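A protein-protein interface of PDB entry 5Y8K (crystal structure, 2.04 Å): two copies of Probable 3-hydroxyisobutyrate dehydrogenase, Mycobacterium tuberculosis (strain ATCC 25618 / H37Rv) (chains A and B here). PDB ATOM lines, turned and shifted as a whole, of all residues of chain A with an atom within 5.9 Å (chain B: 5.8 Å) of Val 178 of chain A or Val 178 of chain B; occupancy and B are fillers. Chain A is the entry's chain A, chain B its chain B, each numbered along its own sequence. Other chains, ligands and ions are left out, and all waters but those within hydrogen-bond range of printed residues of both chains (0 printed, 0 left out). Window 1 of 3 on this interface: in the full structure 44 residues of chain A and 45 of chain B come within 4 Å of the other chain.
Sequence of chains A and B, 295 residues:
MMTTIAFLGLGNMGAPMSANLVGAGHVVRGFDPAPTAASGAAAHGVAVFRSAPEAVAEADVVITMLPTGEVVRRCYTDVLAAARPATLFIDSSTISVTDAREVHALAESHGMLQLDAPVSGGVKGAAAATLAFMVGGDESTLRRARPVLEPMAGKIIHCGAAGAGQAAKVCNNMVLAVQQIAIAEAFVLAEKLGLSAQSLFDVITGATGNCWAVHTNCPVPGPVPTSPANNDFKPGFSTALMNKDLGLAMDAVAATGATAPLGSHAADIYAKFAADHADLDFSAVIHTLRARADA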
ATOM      1  N   ASN A 173      -3.966  33.837  -6.757  1.00  0.00           N
ATOM      2  CA  ASN A 173      -3.217  34.735  -7.657  1.00  0.00           C
ATOM      3  C   ASN A 173      -1.708  34.447  -7.721  1.00  0.00           C
ATOM      4  O   ASN A 173      -1.088  34.669  -8.765  1.00  0.00           O
ATOM      5  CB  ASN A 173      -3.508  36.223  -7.371  1.00  0.00           C
ATOM      6  CG  ASN A 173      -4.876  36.657  -7.888  1.00  0.00           C
ATOM      7  OD1 ASN A 173      -5.788  35.838  -8.067  1.00  0.00           O
ATOM      8  ND2 ASN A 173      -5.035  37.938  -8.106  1.00  0.00           N
ATOM      9  N   MET A 174      -1.135  33.917  -6.636  1.00  0.00           N
ATOM     10  CA  MET A 174       0.257  33.479  -6.662  1.00  0.00           C
ATOM     11  C   MET A 174       0.417  32.279  -7.599  1.00  0.00           C
ATOM     12  O   MET A 174       1.371  32.224  -8.373  1.00  0.00           O
ATOM     13  CB  MET A 174       0.751  33.103  -5.262  1.00  0.00           C
ATOM     14  CG  MET A 174       2.208  32.673  -5.220  1.00  0.00           C
ATOM     15  SD  MET A 174       2.841  32.498  -3.547  1.00  0.00           S
ATOM     16  CE  MET A 174       1.982  31.024  -3.014  1.00  0.00           C
ATOM     17  N   VAL A 175      -0.519  31.329  -7.523  1.00  0.00           N
ATOM     18  CA  VAL A 175      -0.511  30.181  -8.440  1.00  0.00           C
ATOM     19  C   VAL A 175      -0.666  30.665  -9.881  1.00  0.00           C
ATOM     20  O   VAL A 175       0.042  30.185 -10.765  1.00  0.00           O
ATOM     21  CB  VAL A 175      -1.610  29.148  -8.087  1.00  0.00           C
ATOM     22  CG1 VAL A 175      -1.808  28.115  -9.191  1.00  0.00           C
ATOM     23  CG2 VAL A 175      -1.270  28.460  -6.779  1.00  0.00           C
ATOM     24  N   LEU A 176      -1.592  31.606 -10.103  1.00  0.00           N
ATOM     25  CA  LEU A 176      -1.882  32.123 -11.445  1.00  0.00           C
ATOM     26  C   LEU A 176      -0.651  32.745 -12.090  1.00  0.00           C
ATOM     27  O   LEU A 176      -0.398  32.528 -13.262  1.00  0.00           O
ATOM     28  CB  LEU A 176      -3.024  33.146 -11.397  1.00  0.00           C
ATOM     29  CG  LEU A 176      -3.402  33.826 -12.720  1.00  0.00           C
ATOM     30  CD1 LEU A 176      -3.851  32.815 -13.766  1.00  0.00           C
ATOM     31  CD2 LEU A 176      -4.491  34.849 -12.484  1.00  0.00           C
ATOM     32  N   ALA A 177       0.086  33.549 -11.323  1.00  0.00           N
ATOM     33  CA  ALA A 177       1.295  34.193 -11.817  1.00  0.00           C
ATOM     34  C   ALA A 177       2.319  33.154 -12.251  1.00  0.00           C
ATOM     35  O   ALA A 177       2.922  33.281 -13.319  1.00  0.00           O
ATOM     36  CB  ALA A 177       1.903  35.095 -10.750  1.00  0.00           C
ATOM     37  N   VAL A 178       2.513  32.138 -11.422  1.00  0.00           N
ATOM     38  CA  VAL A 178       3.455  31.045 -11.732  1.00  0.00           C
ATOM     39  C   VAL A 178       3.026  30.330 -13.017  1.00  0.00           C
ATOM     40  O   VAL A 178       3.850  30.078 -13.901  1.00  0.00           O
ATOM     41  CB  VAL A 178       3.540  30.021 -10.577  1.00  0.00           C
ATOM     42  CG1 VAL A 178       4.331  28.767 -10.996  1.00  0.00           C
ATOM     43  CG2 VAL A 178       4.157  30.657  -9.330  1.00  0.00           C
ATOM     44  N   GLN A 179       1.730  30.049 -13.119  1.00  0.00           N
ATOM     45  CA  GLN A 179       1.145  29.384 -14.300  1.00  0.00           C
ATOM     46  C   GLN A 179       1.307  30.205 -15.565  1.00  0.00           C
ATOM     47  O   GLN A 179       1.620  29.644 -16.616  1.00  0.00           O
ATOM     48  CB  GLN A 179      -0.341  29.070 -14.093  1.00  0.00           C
ATOM     49  CG  GLN A 179      -0.609  27.988 -13.068  1.00  0.00           C
ATOM     50  CD  GLN A 179      -2.072  27.878 -12.663  1.00  0.00           C
ATOM     51  OE1 GLN A 179      -2.826  28.851 -12.741  1.00  0.00           O
ATOM     52  NE2 GLN A 179      -2.488  26.668 -12.234  1.00  0.00           N
ATOM     53  N   GLN A 180       1.072  31.518 -15.470  1.00  0.00           N
ATOM     54  CA  GLN A 180       1.201  32.396 -16.644  1.00  0.00           C
ATOM     55  C   GLN A 180       2.642  32.461 -17.171  1.00  0.00           C
ATOM     56  O   GLN A 180       2.853  32.490 -18.373  1.00  0.00           O
ATOM     57  CB  GLN A 180       0.665  33.795 -16.357  1.00  0.00           C
ATOM     58  CG  GLN A 180       0.404  34.629 -17.599  1.00  0.00           C
ATOM     59  CD  GLN A 180      -0.741  34.112 -18.446  1.00  0.00           C
ATOM     60  OE1 GLN A 180      -1.896  34.170 -18.041  1.00  0.00           O
ATOM     61  NE2 GLN A 180      -0.426  33.597 -19.620  1.00  0.00           N
ATOM     62  N   ILE A 181       3.620  32.471 -16.267  1.00  0.00           N
ATOM     63  CA  ILE A 181       5.023  32.443 -16.668  1.00  0.00           C
ATOM     64  C   ILE A 181       5.368  31.071 -17.252  1.00  0.00           C
ATOM     65  O   ILE A 181       6.004  30.981 -18.305  1.00  0.00           O
ATOM     66  CB  ILE A 181       5.957  32.816 -15.499  1.00  0.00           C
ATOM     67  CG1 ILE A 181       5.708  34.274 -15.075  1.00  0.00           C
ATOM     68  CG2 ILE A 181       7.409  32.618 -15.894  1.00  0.00           C
ATOM     69  CD1 ILE A 181       6.138  34.585 -13.659  1.00  0.00           C
ATOM     70  N   ALA A 182       4.919  30.019 -16.578  1.00  0.00           N
ATOM     71  CA  ALA A 182       5.183  28.637 -17.003  1.00  0.00           C
ATOM     72  C   ALA A 182       4.659  28.344 -18.411  1.00  0.00           C
ATOM     73  O   ALA A 182       5.369  27.762 -19.232  1.00  0.00           O
ATOM     74  CB  ALA A 182       4.589  27.661 -16.004  1.00  0.00           C
ATOM     75  N   ILE A 183       3.425  28.764 -18.678  1.00  0.00           N
ATOM     76  CA  ILE A 183       2.841  28.657 -20.017  1.00  0.00           C
ATOM     77  C   ILE A 183       3.681  29.433 -21.038  1.00  0.00           C
ATOM     78  O   ILE A 183       3.956  28.915 -22.122  1.00  0.00           O
ATOM     79  CB  ILE A 183       1.354  29.118 -20.008  1.00  0.00           C
ATOM     80  CG1 ILE A 183       0.500  28.099 -19.241  1.00  0.00           C
ATOM     81  CG2 ILE A 183       0.799  29.390 -21.400  1.00  0.00           C
ATOM     82  CD1 ILE A 183       0.487  26.702 -19.795  1.00  0.00           C
ATOM     83  N   GLU A 185       6.896  30.136 -20.922  1.00  0.00           N
ATOM     84  CA  GLU A 185       8.131  29.382 -21.130  1.00  0.00           C
ATOM     85  C   GLU A 185       7.903  28.218 -22.088  1.00  0.00           C
ATOM     86  O   GLU A 185       8.712  27.992 -22.999  1.00  0.00           O
ATOM     87  CB  GLU A 185       8.679  28.835 -19.819  1.00  0.00           C
ATOM     88  CG  GLU A 185       9.121  29.880 -18.813  1.00  0.00           C
ATOM     89  CD  GLU A 185       9.490  29.276 -17.455  1.00  0.00           C
ATOM     90  OE1 GLU A 185       9.644  28.027 -17.309  1.00  0.00           O
ATOM     91  OE2 GLU A 185       9.651  30.064 -16.512  1.00  0.00           O
ATOM     92  N   LEU A 262       8.818  29.078  -6.074  1.00  0.00           N
ATOM     93  CA  LEU A 262       8.343  29.463  -7.413  1.00  0.00           C
ATOM     94  C   LEU A 262       7.454  30.706  -7.376  1.00  0.00           C
ATOM     95  O   LEU A 262       7.565  31.567  -8.236  1.00  0.00           O
ATOM     96  CB  LEU A 262       7.627  28.311  -8.110  1.00  0.00           C
ATOM     97  CG  LEU A 262       8.465  27.038  -8.307  1.00  0.00           C
ATOM     98  CD1 LEU A 262       7.672  26.041  -9.134  1.00  0.00           C
ATOM     99  CD2 LEU A 262       9.819  27.313  -8.964  1.00  0.00           C
ATOM    100  N   GLY A 263       6.581  30.797  -6.381  1.00  0.00           N
ATOM    101  CA  GLY A 263       5.784  31.994  -6.165  1.00  0.00           C
ATOM    102  C   GLY A 263       6.643  33.231  -5.943  1.00  0.00           C
ATOM    103  O   GLY A 263       6.365  34.276  -6.513  1.00  0.00           O
ATOM    104  N   ALA A 266       8.311  34.064  -9.246  1.00  0.00           N
ATOM    105  CA  ALA A 266       7.293  34.740 -10.063  1.00  0.00           C
ATOM    106  C   ALA A 266       7.128  36.188  -9.632  1.00  0.00           C
ATOM    107  O   ALA A 266       6.980  37.070 -10.461  1.00  0.00           O
ATOM    108  CB  ALA A 266       5.961  34.010  -9.972  1.00  0.00           C
ATOM    109  N   TYR A 270       7.759  39.433 -12.051  1.00  0.00           N
ATOM    110  CA  TYR A 270       6.720  40.428 -12.333  1.00  0.00           C
ATOM    111  C   TYR A 270       7.036  41.827 -11.793  1.00  0.00           C
ATOM    112  O   TYR A 270       6.606  42.794 -12.388  1.00  0.00           O
ATOM    113  CB  TYR A 270       5.344  39.954 -11.859  1.00  0.00           C
ATOM    114  CG  TYR A 270       4.629  39.123 -12.893  1.00  0.00           C
ATOM    115  CD1 TYR A 270       4.257  39.684 -14.108  1.00  0.00           C
ATOM    116  CD2 TYR A 270       4.306  37.775 -12.658  1.00  0.00           C
ATOM    117  CE1 TYR A 270       3.602  38.941 -15.074  1.00  0.00           C
ATOM    118  CE2 TYR A 270       3.650  37.018 -13.624  1.00  0.00           C
ATOM    119  CZ  TYR A 270       3.299  37.608 -14.833  1.00  0.00           C
ATOM    120  OH  TYR A 270       2.643  36.891 -15.807  1.00  0.00           O
ATOM    121  N   ASN B 173       4.880  18.493 -19.619  1.00  0.00           N
ATOM    122  CA  ASN B 173       5.328  17.967 -18.322  1.00  0.00           C
ATOM    123  C   ASN B 173       6.215  18.956 -17.544  1.00  0.00           C
ATOM    124  O   ASN B 173       6.281  18.891 -16.320  1.00  0.00           O
ATOM    125  CB  ASN B 173       5.995  16.589 -18.478  1.00  0.00           C
ATOM    126  CG  ASN B 173       4.990  15.467 -18.794  1.00  0.00           C
ATOM    127  OD1 ASN B 173       3.817  15.707 -19.133  1.00  0.00           O
ATOM    128  ND2 ASN B 173       5.455  14.234 -18.697  1.00  0.00           N
ATOM    129  N   MET B 174       6.872  19.883 -18.232  1.00  0.00           N
ATOM    130  CA  MET B 174       7.574  20.964 -17.543  1.00  0.00           C
ATOM    131  C   MET B 174       6.544  21.873 -16.839  1.00  0.00           C
ATOM    132  O   MET B 174       6.693  22.200 -15.668  1.00  0.00           O
ATOM    133  CB  MET B 174       8.427  21.780 -18.530  1.00  0.00           C
ATOM    134  CG  MET B 174       9.298  22.851 -17.877  1.00  0.00           C
ATOM    135  SD  MET B 174      10.452  23.729 -18.960  1.00  0.00           S
ATOM    136  CE  MET B 174       9.356  24.642 -20.044  1.00  0.00           C
ATOM    137  N   VAL B 175       5.493  22.242 -17.564  1.00  0.00           N
ATOM    138  CA  VAL B 175       4.405  23.053 -17.004  1.00  0.00           C
ATOM    139  C   VAL B 175       3.787  22.329 -15.807  1.00  0.00           C
ATOM    140  O   VAL B 175       3.617  22.925 -14.744  1.00  0.00           O
ATOM    141  CB  VAL B 175       3.320  23.383 -18.051  1.00  0.00           C
ATOM    142  CG1 VAL B 175       2.152  24.097 -17.405  1.00  0.00           C
ATOM    143  CG2 VAL B 175       3.884  24.240 -19.162  1.00  0.00           C
ATOM    144  N   LEU B 176       3.500  21.040 -15.978  1.00  0.00           N
ATOM    145  CA  LEU B 176       2.941  20.226 -14.910  1.00  0.00           C
ATOM    146  C   LEU B 176       3.779  20.256 -13.623  1.00  0.00           C
ATOM    147  O   LEU B 176       3.239  20.453 -12.536  1.00  0.00           O
ATOM    148  CB  LEU B 176       2.766  18.784 -15.384  1.00  0.00           C
ATOM    149  CG  LEU B 176       2.238  17.796 -14.331  1.00  0.00           C
ATOM    150  CD1 LEU B 176       0.873  18.252 -13.815  1.00  0.00           C
ATOM    151  CD2 LEU B 176       2.188  16.393 -14.927  1.00  0.00           C
ATOM    152  N   ALA B 177       5.087  20.054 -13.770  1.00  0.00           N
ATOM    153  CA  ALA B 177       6.048  20.112 -12.669  1.00  0.00           C
ATOM    154  C   ALA B 177       5.983  21.440 -11.921  1.00  0.00           C
ATOM    155  O   ALA B 177       5.892  21.455 -10.705  1.00  0.00           O
ATOM    156  CB  ALA B 177       7.457  19.888 -13.187  1.00  0.00           C
ATOM    157  N   VAL B 178       6.009  22.532 -12.674  1.00  0.00           N
ATOM    158  CA  VAL B 178       5.893  23.891 -12.126  1.00  0.00           C
ATOM    159  C   VAL B 178       4.541  24.076 -11.396  1.00  0.00           C
ATOM    160  O   VAL B 178       4.488  24.606 -10.290  1.00  0.00           O
ATOM    161  CB  VAL B 178       6.079  24.945 -13.245  1.00  0.00           C
ATOM    162  CG1 VAL B 178       5.720  26.355 -12.773  1.00  0.00           C
ATOM    163  CG2 VAL B 178       7.504  24.926 -13.787  1.00  0.00           C
ATOM    164  N   GLN B 179       3.458  23.625 -12.018  1.00  0.00           N
ATOM    165  CA  GLN B 179       2.140  23.688 -11.402  1.00  0.00           C
ATOM    166  C   GLN B 179       2.031  22.863 -10.124  1.00  0.00           C
ATOM    167  O   GLN B 179       1.407  23.290  -9.174  1.00  0.00           O
ATOM    168  CB  GLN B 179       1.055  23.234 -12.396  1.00  0.00           C
ATOM    169  CG  GLN B 179       0.826  24.195 -13.550  1.00  0.00           C
ATOM    170  CD  GLN B 179      -0.012  23.588 -14.662  1.00  0.00           C
ATOM    171  OE1 GLN B 179      -0.052  22.368 -14.816  1.00  0.00           O
ATOM    172  NE2 GLN B 179      -0.671  24.439 -15.459  1.00  0.00           N
ATOM    173  N   GLN B 180       2.637  21.685 -10.090  1.00  0.00           N
ATOM    174  CA  GLN B 180       2.518  20.822  -8.915  1.00  0.00           C
ATOM    175  C   GLN B 180       3.276  21.394  -7.729  1.00  0.00           C
ATOM    176  O   GLN B 180       2.793  21.307  -6.591  1.00  0.00           O
ATOM    177  CB  GLN B 180       2.974  19.389  -9.215  1.00  0.00           C
ATOM    178  CG  GLN B 180       2.602  18.361  -8.155  1.00  0.00           C
ATOM    179  CD  GLN B 180       1.110  18.100  -8.078  1.00  0.00           C
ATOM    180  OE1 GLN B 180       0.504  17.568  -9.016  1.00  0.00           O
ATOM    181  NE2 GLN B 180       0.503  18.496  -6.971  1.00  0.00           N
ATOM    182  N   ILE B 181       4.434  21.997  -7.982  1.00  0.00           N
ATOM    183  CA  ILE B 181       5.155  22.739  -6.927  1.00  0.00           C
ATOM    184  C   ILE B 181       4.333  23.966  -6.464  1.00  0.00           C
ATOM    185  O   ILE B 181       4.167  24.193  -5.265  1.00  0.00           O
ATOM    186  CB  ILE B 181       6.573  23.156  -7.389  1.00  0.00           C
ATOM    187  CG1 ILE B 181       7.460  21.913  -7.609  1.00  0.00           C
ATOM    188  CG2 ILE B 181       7.235  24.050  -6.358  1.00  0.00           C
ATOM    189  CD1 ILE B 181       8.740  22.186  -8.388  1.00  0.00           C
ATOM    190  N   ALA B 182       3.811  24.734  -7.410  1.00  0.00           N
ATOM    191  CA  ALA B 182       3.067  25.960  -7.090  1.00  0.00           C
ATOM    192  C   ALA B 182       1.798  25.697  -6.295  1.00  0.00           C
ATOM    193  O   ALA B 182       1.493  26.440  -5.367  1.00  0.00           O
ATOM    194  CB  ALA B 182       2.729  26.738  -8.359  1.00  0.00           C
ATOM    195  N   ILE B 183       1.061  24.654  -6.666  1.00  0.00           N
ATOM    196  CA  ILE B 183      -0.099  24.226  -5.889  1.00  0.00           C
ATOM    197  C   ILE B 183       0.332  23.814  -4.479  1.00  0.00           C
ATOM    198  O   ILE B 183      -0.345  24.131  -3.518  1.00  0.00           O
ATOM    199  CB  ILE B 183      -0.895  23.097  -6.595  1.00  0.00           C
ATOM    200  CG1 ILE B 183      -1.616  23.629  -7.850  1.00  0.00           C
ATOM    201  CG2 ILE B 183      -1.875  22.413  -5.652  1.00  0.00           C
ATOM    202  CD1 ILE B 183      -2.699  24.668  -7.608  1.00  0.00           C
ATOM    203  N   GLU B 185       2.917  24.950  -2.757  1.00  0.00           N
ATOM    204  CA  GLU B 185       3.261  26.186  -2.056  1.00  0.00           C
ATOM    205  C   GLU B 185       1.995  26.885  -1.548  1.00  0.00           C
ATOM    206  O   GLU B 185       1.923  27.298  -0.395  1.00  0.00           O
ATOM    207  CB  GLU B 185       4.028  27.132  -2.976  1.00  0.00           C
ATOM    208  CG  GLU B 185       5.395  26.627  -3.428  1.00  0.00           C
ATOM    209  CD  GLU B 185       6.097  27.571  -4.407  1.00  0.00           C
ATOM    210  OE1 GLU B 185       5.593  28.688  -4.687  1.00  0.00           O
ATOM    211  OE2 GLU B 185       7.196  27.212  -4.883  1.00  0.00           O
ATOM    212  N   LEU B 262      11.277  29.313 -14.328  1.00  0.00           N
ATOM    213  CA  LEU B 262      10.522  28.505 -13.374  1.00  0.00           C
ATOM    214  C   LEU B 262      10.619  27.043 -13.698  1.00  0.00           C
ATOM    215  O   LEU B 262      10.692  26.208 -12.797  1.00  0.00           O
ATOM    216  CB  LEU B 262       9.055  28.937 -13.313  1.00  0.00           C
ATOM    217  CG  LEU B 262       8.804  30.413 -13.014  1.00  0.00           C
ATOM    218  CD1 LEU B 262       7.332  30.657 -12.676  1.00  0.00           C
ATOM    219  CD2 LEU B 262       9.698  30.897 -11.889  1.00  0.00           C
ATOM    220  N   GLY B 263      10.609  26.725 -14.989  1.00  0.00           N
ATOM    221  CA  GLY B 263      10.839  25.359 -15.438  1.00  0.00           C
ATOM    222  C   GLY B 263      12.180  24.816 -14.966  1.00  0.00           C
ATOM    223  O   GLY B 263      12.248  23.699 -14.480  1.00  0.00           O
ATOM    224  N   ALA B 266      11.984  24.415 -11.159  1.00  0.00           N
ATOM    225  CA  ALA B 266      11.263  23.195 -10.865  1.00  0.00           C
ATOM    226  C   ALA B 266      12.137  21.962 -11.075  1.00  0.00           C
ATOM    227  O   ALA B 266      12.079  21.037 -10.273  1.00  0.00           O
ATOM    228  CB  ALA B 266       9.995  23.111 -11.699  1.00  0.00           C
ATOM    229  N   TYR B 270      12.962  19.221  -8.234  1.00  0.00           N
ATOM    230  CA  TYR B 270      12.690  17.785  -8.382  1.00  0.00           C
ATOM    231  C   TYR B 270      13.960  16.922  -8.392  1.00  0.00           C
ATOM    232  O   TYR B 270      13.925  15.793  -7.912  1.00  0.00           O
ATOM    233  CB  TYR B 270      11.788  17.486  -9.587  1.00  0.00           C
ATOM    234  CG  TYR B 270      10.326  17.575  -9.206  1.00  0.00           C
ATOM    235  CD1 TYR B 270       9.773  16.645  -8.332  1.00  0.00           C
ATOM    236  CD2 TYR B 270       9.510  18.617  -9.676  1.00  0.00           C
ATOM    237  CE1 TYR B 270       8.448  16.721  -7.959  1.00  0.00           C
ATOM    238  CE2 TYR B 270       8.181  18.708  -9.304  1.00  0.00           C
ATOM    239  CZ  TYR B 270       7.657  17.761  -8.449  1.00  0.00           C
ATOM    240  OH  TYR B 270       6.344  17.833  -8.074  1.00  0.00           O
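The side-chain carboxylate of Glu 185 of chain A lies within hydrogen-bond range of the backbone NH of Gly 263 of chain B, 2.8 Å away. The side-chain carboxylate (OE2) of Glu 185 of chain A lies within hydrogen-bond range of the backbone NH (N) of Leu 262 of chain B, at 2.8 Å. N of Gly 263 of chain A is in hydrogen-bond range of OE1 of Glu 185 of chain B (2.9 Å). The backbone NH of Leu 262 of chain A is in hydrogen-bond range of the side-chain carboxylate of Glu 185 of chain B, at 2.7 Å.
Asn 173 of chain A touches none of the printed residues of chain B. Printed residues of chain B within 4 Å of Val 175 of chain A: Ala 182 (3.7 Å) and Ile 183 (3.9 Å). Of chain B, only Val 178 (3.3 Å), Ala 182 (3.7 Å) and Leu 262 (3.7 Å) come within 4 Å of Val 178 of chain A. Printed residues of chain B within 4 Å of Ala 182 of chain A: Val 175 and Val 178. Printed residues of chain B within 4 Å of Glu 185 of chain A: Leu 262 and Gly 263. Of the printed residues of chain B, Gly 263 of chain A touches Glu 185. Of the printed residues of chain A, Ile 183 of chain B touches Val 175. The nearest residue of chain A that does not touch Val 178 of chain B is Glu 185 of chain A (5.2 Å). The nearest printed residue of chain A that does not touch Gly 263 of chain B is Ala 182 of chain A (6.1 Å).
Ala 182 of chain B touches Val 175 of chain A. Val 175 of chain A touches Ile 183 of chain B. CB of Ala 182 of chain B touches CG1 of Val 178 of chain A (3.7 Å). Val 178 of chain A touches Leu 262 of chain B (O to CD1, 3.7 Å). CD1 of Leu 262 of chain B touches CG2 of Ile 181 of chain A, 3.8 Å away. Ala 182 of chain A touches Val 175 of chain B (O to CG2, 3.8 Å). CG1 of Val 178 of chain B touches CB of Ala 182 of chain A (3.7 Å). Val 175 of chain B touches Ile 183 of chain A. Leu 262 of chain A touches Val 178 of chain B (CD1 to O, 3.7 Å). CD1 of Leu 262 of chain A touches CG2 of Ile 181 of chain B, 3.4 Å away.
Of the 16 printed residues of chain B, 8 touch a printed residue of chain A. Printed residues of chain B that touch a printed residue of chain A: Val 175, Val 178, Ile 181, Ala 182, Ile 183, Glu 185, Leu 262 and Gly 263. Hydrophobic or aromatic side chains of chain B within 4 Å of the printed part of chain A: Val 175, Val 178, Ile 181, Ala 182, Ile 183 and Leu 262. Along chain B the printed residues that touch a printed residue of chain A span positions 175 to 263. Along chain A the printed residues that touch a printed residue of chain B span positions 175 to 263. Among the printed residues, no Asp or Glu carboxylate lies within 4 Å of a Lys or Arg side-chain nitrogen of the other chain.
Val 178 of chain A touches Ala 182 of chain B, and with the chains exchanged Ala 182 of chain A touches Val 178 of chain B. Ile 181 of chain A touches Leu 262 of chain B, and with the chains exchanged Leu 262 of chain A touches Ile 181 of chain B. Glu 185 of chain A touches Leu 262 of chain B, and with the chains exchanged Leu 262 of chain A touches Glu 185 of chain B. Glu 185 of chain A touches Gly 263 of chain B, and with the chains exchanged Gly 263 of chain A touches Glu 185 of chain B. Positions printed for both chains: 173, 174, 175, 176, 177, 178, 179, 180, 181, 182, 183, 185, 262, 263, 266 and 270.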
